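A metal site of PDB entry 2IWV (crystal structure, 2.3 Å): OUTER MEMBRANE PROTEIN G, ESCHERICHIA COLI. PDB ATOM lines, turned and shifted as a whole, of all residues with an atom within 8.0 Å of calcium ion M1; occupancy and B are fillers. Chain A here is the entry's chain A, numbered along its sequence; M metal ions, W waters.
Calcium ion M1 is bound by water W1 (1.8 Å), the side-chain carboxylate of Asp 26 (2.3 Å), the backbone carbonyl oxygen of Met 27 (2.3 Å), the backbone carbonyl oxygen of Gly 22 (2.4 Å), the backbone carbonyl oxygen of Val 20 (2.4 Å), the side-chain amide oxygen of Asn 19 (2.5 Å) and water W2 (2.6 Å).
The side-chain sulfur (SD) of Met 27 lies within hydrogen-bond range of the side-chain hydroxyl (OH) of Tyr 23, 3.3 Å away. The side-chain amide oxygen (OD1) of Asn 19 lies close to the backbone NH (N) of Gly 29 (2.9 Å). O of Asp 28 sits close to OD1 of Asn 19, at 3.1 Å. The backbone NH (N) of Val 56 lies within hydrogen-bond range of the backbone carbonyl oxygen (O) of Gly 29.
Merely in contact with calcium ion M1: Gly 29 (3.9 Å). Along chain A the residues within 4 Å of calcium ion M1 span positions 19 to 29.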
ATOM      1  N   GLU A  18     -20.283   5.701  23.205  1.00  0.00           N
ATOM      2  CA  GLU A  18     -20.669   4.449  23.884  1.00  0.00           C
ATOM      3  C   GLU A  18     -19.462   3.563  24.055  1.00  0.00           C
ATOM      4  O   GLU A  18     -18.709   3.361  23.111  1.00  0.00           O
ATOM      5  CB  GLU A  18     -21.692   3.680  23.077  1.00  0.00           C
ATOM      6  CG  GLU A  18     -22.992   4.416  22.930  1.00  0.00           C
ATOM      7  CD  GLU A  18     -23.937   3.713  21.933  1.00  0.00           C
ATOM      8  OE1 GLU A  18     -23.601   3.642  20.699  1.00  0.00           O
ATOM      9  OE2 GLU A  18     -25.010   3.227  22.412  1.00  0.00           O
ATOM     10  N   ASN A  19     -19.275   3.036  25.263  1.00  0.00           N
ATOM     11  CA  ASN A  19     -18.032   2.324  25.535  1.00  0.00           C
ATOM     12  C   ASN A  19     -18.207   1.342  26.685  1.00  0.00           C
ATOM     13  O   ASN A  19     -18.667   1.770  27.738  1.00  0.00           O
ATOM     14  CB  ASN A  19     -16.894   3.360  25.837  1.00  0.00           C
ATOM     15  CG  ASN A  19     -15.609   2.735  26.351  1.00  0.00           C
ATOM     16  OD1 ASN A  19     -14.869   2.029  25.634  1.00  0.00           O
ATOM     17  ND2 ASN A  19     -15.339   2.959  27.618  1.00  0.00           N
ATOM     18  N   VAL A  20     -17.887   0.065  26.427  1.00  0.00           N
ATOM     19  CA  VAL A  20     -17.777  -1.002  27.417  1.00  0.00           C
ATOM     20  C   VAL A  20     -16.367  -0.935  27.955  1.00  0.00           C
ATOM     21  O   VAL A  20     -15.405  -0.995  27.177  1.00  0.00           O
ATOM     22  CB  VAL A  20     -17.925  -2.378  26.756  1.00  0.00           C
ATOM     23  CG1 VAL A  20     -17.885  -3.486  27.766  1.00  0.00           C
ATOM     24  CG2 VAL A  20     -19.251  -2.457  25.985  1.00  0.00           C
ATOM     25  N   GLU A  21     -16.203  -0.794  29.292  1.00  0.00           N
ATOM     26  CA  GLU A  21     -14.863  -0.536  29.722  1.00  0.00           C
ATOM     27  C   GLU A  21     -13.990  -1.756  29.634  1.00  0.00           C
ATOM     28  O   GLU A  21     -14.480  -2.900  29.652  1.00  0.00           O
ATOM     29  CB  GLU A  21     -14.772   0.247  31.004  1.00  0.00           C
ATOM     30  CG  GLU A  21     -15.808  -0.123  32.042  1.00  0.00           C
ATOM     31  CD  GLU A  21     -15.471   0.483  33.377  1.00  0.00           C
ATOM     32  OE1 GLU A  21     -14.469   0.052  34.000  1.00  0.00           O
ATOM     33  OE2 GLU A  21     -16.196   1.406  33.816  1.00  0.00           O
ATOM     34  N   GLY A  22     -12.707  -1.515  29.415  1.00  0.00           N
ATOM     35  CA  GLY A  22     -11.813  -2.521  28.868  1.00  0.00           C
ATOM     36  C   GLY A  22     -11.564  -2.181  27.413  1.00  0.00           C
ATOM     37  O   GLY A  22     -12.326  -1.417  26.795  1.00  0.00           O
ATOM     38  N   TYR A  23     -10.493  -2.740  26.873  1.00  0.00           N
ATOM     39  CA  TYR A  23     -10.140  -2.575  25.464  1.00  0.00           C
ATOM     40  C   TYR A  23     -10.622  -3.803  24.710  1.00  0.00           C
ATOM     41  O   TYR A  23      -9.850  -4.684  24.304  1.00  0.00           O
ATOM     42  CB  TYR A  23      -8.627  -2.405  25.311  1.00  0.00           C
ATOM     43  CG  TYR A  23      -8.180  -1.858  23.986  1.00  0.00           C
ATOM     44  CD1 TYR A  23      -8.145  -0.485  23.754  1.00  0.00           C
ATOM     45  CD2 TYR A  23      -7.788  -2.712  22.964  1.00  0.00           C
ATOM     46  CE1 TYR A  23      -7.723   0.012  22.545  1.00  0.00           C
ATOM     47  CE2 TYR A  23      -7.374  -2.229  21.740  1.00  0.00           C
ATOM     48  CZ  TYR A  23      -7.349  -0.869  21.534  1.00  0.00           C
ATOM     49  OH  TYR A  23      -6.952  -0.405  20.290  1.00  0.00           O
ATOM     50  N   GLY A  24     -11.948  -3.856  24.587  1.00  0.00           N
ATOM     51  CA  GLY A  24     -12.671  -4.945  23.983  1.00  0.00           C
ATOM     52  C   GLY A  24     -12.831  -4.625  22.527  1.00  0.00           C
ATOM     53  O   GLY A  24     -11.955  -3.988  21.925  1.00  0.00           O
ATOM     54  N   GLU A  25     -13.956  -5.053  21.971  1.00  0.00           N
ATOM     55  CA  GLU A  25     -14.197  -4.845  20.549  1.00  0.00           C
ATOM     56  C   GLU A  25     -14.437  -3.364  20.208  1.00  0.00           C
ATOM     57  O   GLU A  25     -14.159  -2.962  19.094  1.00  0.00           O
ATOM     58  CB  GLU A  25     -15.333  -5.797  20.077  1.00  0.00           C
ATOM     59  CG  GLU A  25     -16.190  -5.289  18.938  1.00  0.00           C
ATOM     60  CD  GLU A  25     -16.484  -6.354  17.911  1.00  0.00           C
ATOM     61  OE1 GLU A  25     -16.032  -6.193  16.749  1.00  0.00           O
ATOM     62  OE2 GLU A  25     -17.161  -7.350  18.247  1.00  0.00           O
ATOM     63  N   ASP A  26     -14.906  -2.562  21.170  1.00  0.00           N
ATOM     64  CA  ASP A  26     -15.243  -1.141  20.923  1.00  0.00           C
ATOM     65  C   ASP A  26     -14.143  -0.163  21.290  1.00  0.00           C
ATOM     66  O   ASP A  26     -14.391   0.836  21.919  1.00  0.00           O
ATOM     67  CB  ASP A  26     -16.584  -0.753  21.591  1.00  0.00           C
ATOM     68  CG  ASP A  26     -16.499  -0.527  23.135  1.00  0.00           C
ATOM     69  OD1 ASP A  26     -17.588  -0.382  23.779  1.00  0.00           O
ATOM     70  OD2 ASP A  26     -15.403  -0.491  23.732  1.00  0.00           O
ATOM     71  N   MET A  27     -12.968  -0.427  20.810  1.00  0.00           N
ATOM     72  CA  MET A  27     -11.734  -0.291  21.593  1.00  0.00           C
ATOM     73  C   MET A  27     -11.768   0.604  22.836  1.00  0.00           C
ATOM     74  O   MET A  27     -12.142   0.122  23.901  1.00  0.00           O
ATOM     75  CB  MET A  27     -10.597   0.055  20.659  1.00  0.00           C
ATOM     76  CG  MET A  27     -10.621  -0.799  19.431  1.00  0.00           C
ATOM     77  SD  MET A  27      -9.534  -0.209  18.180  1.00  0.00           S
ATOM     78  CE  MET A  27     -10.482   0.712  17.043  1.00  0.00           C
ATOM     79  N   ASP A  28     -11.399   1.883  22.693  1.00  0.00           N
ATOM     80  CA  ASP A  28     -11.562   2.943  23.698  1.00  0.00           C
ATOM     81  C   ASP A  28     -12.966   3.491  23.800  1.00  0.00           C
ATOM     82  O   ASP A  28     -13.229   4.404  24.581  1.00  0.00           O
ATOM     83  CB  ASP A  28     -10.623   4.135  23.423  1.00  0.00           C
ATOM     84  CG  ASP A  28      -9.158   3.840  23.737  1.00  0.00           C
ATOM     85  OD1 ASP A  28      -8.294   4.483  23.111  1.00  0.00           O
ATOM     86  OD2 ASP A  28      -8.866   2.979  24.604  1.00  0.00           O
ATOM     87  N   GLY A  29     -13.891   2.916  23.025  1.00  0.00           N
ATOM     88  CA  GLY A  29     -15.293   3.344  22.944  1.00  0.00           C
ATOM     89  C   GLY A  29     -15.714   3.591  21.502  1.00  0.00           C
ATOM     90  O   GLY A  29     -14.860   3.758  20.604  1.00  0.00           O
ATOM     91  N   LEU A  30     -17.023   3.589  21.293  1.00  0.00           N
ATOM     92  CA  LEU A  30     -17.667   3.911  20.026  1.00  0.00           C
ATOM     93  C   LEU A  30     -17.957   5.409  20.081  1.00  0.00           C
ATOM     94  O   LEU A  30     -18.592   5.853  21.067  1.00  0.00           O
ATOM     95  CB  LEU A  30     -19.010   3.185  19.957  1.00  0.00           C
ATOM     96  CG  LEU A  30     -19.291   1.988  19.056  1.00  0.00           C
ATOM     97  CD1 LEU A  30     -18.199   1.013  19.055  1.00  0.00           C
ATOM     98  CD2 LEU A  30     -20.609   1.280  19.507  1.00  0.00           C
ATOM     99  N   PRO A  55     -15.520   2.118  16.466  1.00  0.00           N
ATOM    100  CA  PRO A  55     -14.598   2.176  17.582  1.00  0.00           C
ATOM    101  C   PRO A  55     -13.339   3.058  17.356  1.00  0.00           C
ATOM    102  O   PRO A  55     -12.921   3.327  16.179  1.00  0.00           O
ATOM    103  CB  PRO A  55     -14.232   0.708  17.844  1.00  0.00           C
ATOM    104  CG  PRO A  55     -14.461   0.012  16.539  1.00  0.00           C
ATOM    105  CD  PRO A  55     -15.535   0.779  15.832  1.00  0.00           C
ATOM    106  N   VAL A  56     -12.767   3.524  18.470  1.00  0.00           N
ATOM    107  CA  VAL A  56     -11.598   4.410  18.413  1.00  0.00           C
ATOM    108  C   VAL A  56     -10.461   3.971  19.314  1.00  0.00           C
ATOM    109  O   VAL A  56     -10.676   3.511  20.439  1.00  0.00           O
ATOM    110  CB  VAL A  56     -11.925   5.945  18.691  1.00  0.00           C
ATOM    111  CG1 VAL A  56     -10.678   6.839  18.433  1.00  0.00           C
ATOM    112  CG2 VAL A  56     -13.065   6.467  17.827  1.00  0.00           C
ATOM    113  N   LYS A 269     -19.333  -3.211  32.232  1.00  0.00           N
ATOM    114  CA  LYS A 269     -19.793  -1.884  32.680  1.00  0.00           C
ATOM    115  C   LYS A 269     -19.759  -0.997  31.460  1.00  0.00           C
ATOM    116  O   LYS A 269     -18.774  -0.931  30.764  1.00  0.00           O
ATOM    117  CB  LYS A 269     -18.892  -1.265  33.770  1.00  0.00           C
ATOM    118  CG  LYS A 269     -18.333  -2.234  34.799  1.00  0.00           C
ATOM    119  CD  LYS A 269     -19.050  -2.154  36.161  1.00  0.00           C
ATOM    120  CE  LYS A 269     -18.422  -1.083  37.039  1.00  0.00           C
ATOM    121  NZ  LYS A 269     -16.917  -1.075  36.912  1.00  0.00           N
HETATM  122 CA    CA M   1     -13.886  -0.218  25.423  1.00  0.00          CA
HETATM  123 CA    CA M   2     -14.469  -4.092  27.166  1.00  0.00          CA
HETATM  124  O   HOH W   1     -12.651   0.930  26.180  1.00  0.00           O
HETATM  125  O   HOH W   2     -14.364  -2.665  24.777  1.00  0.00           O
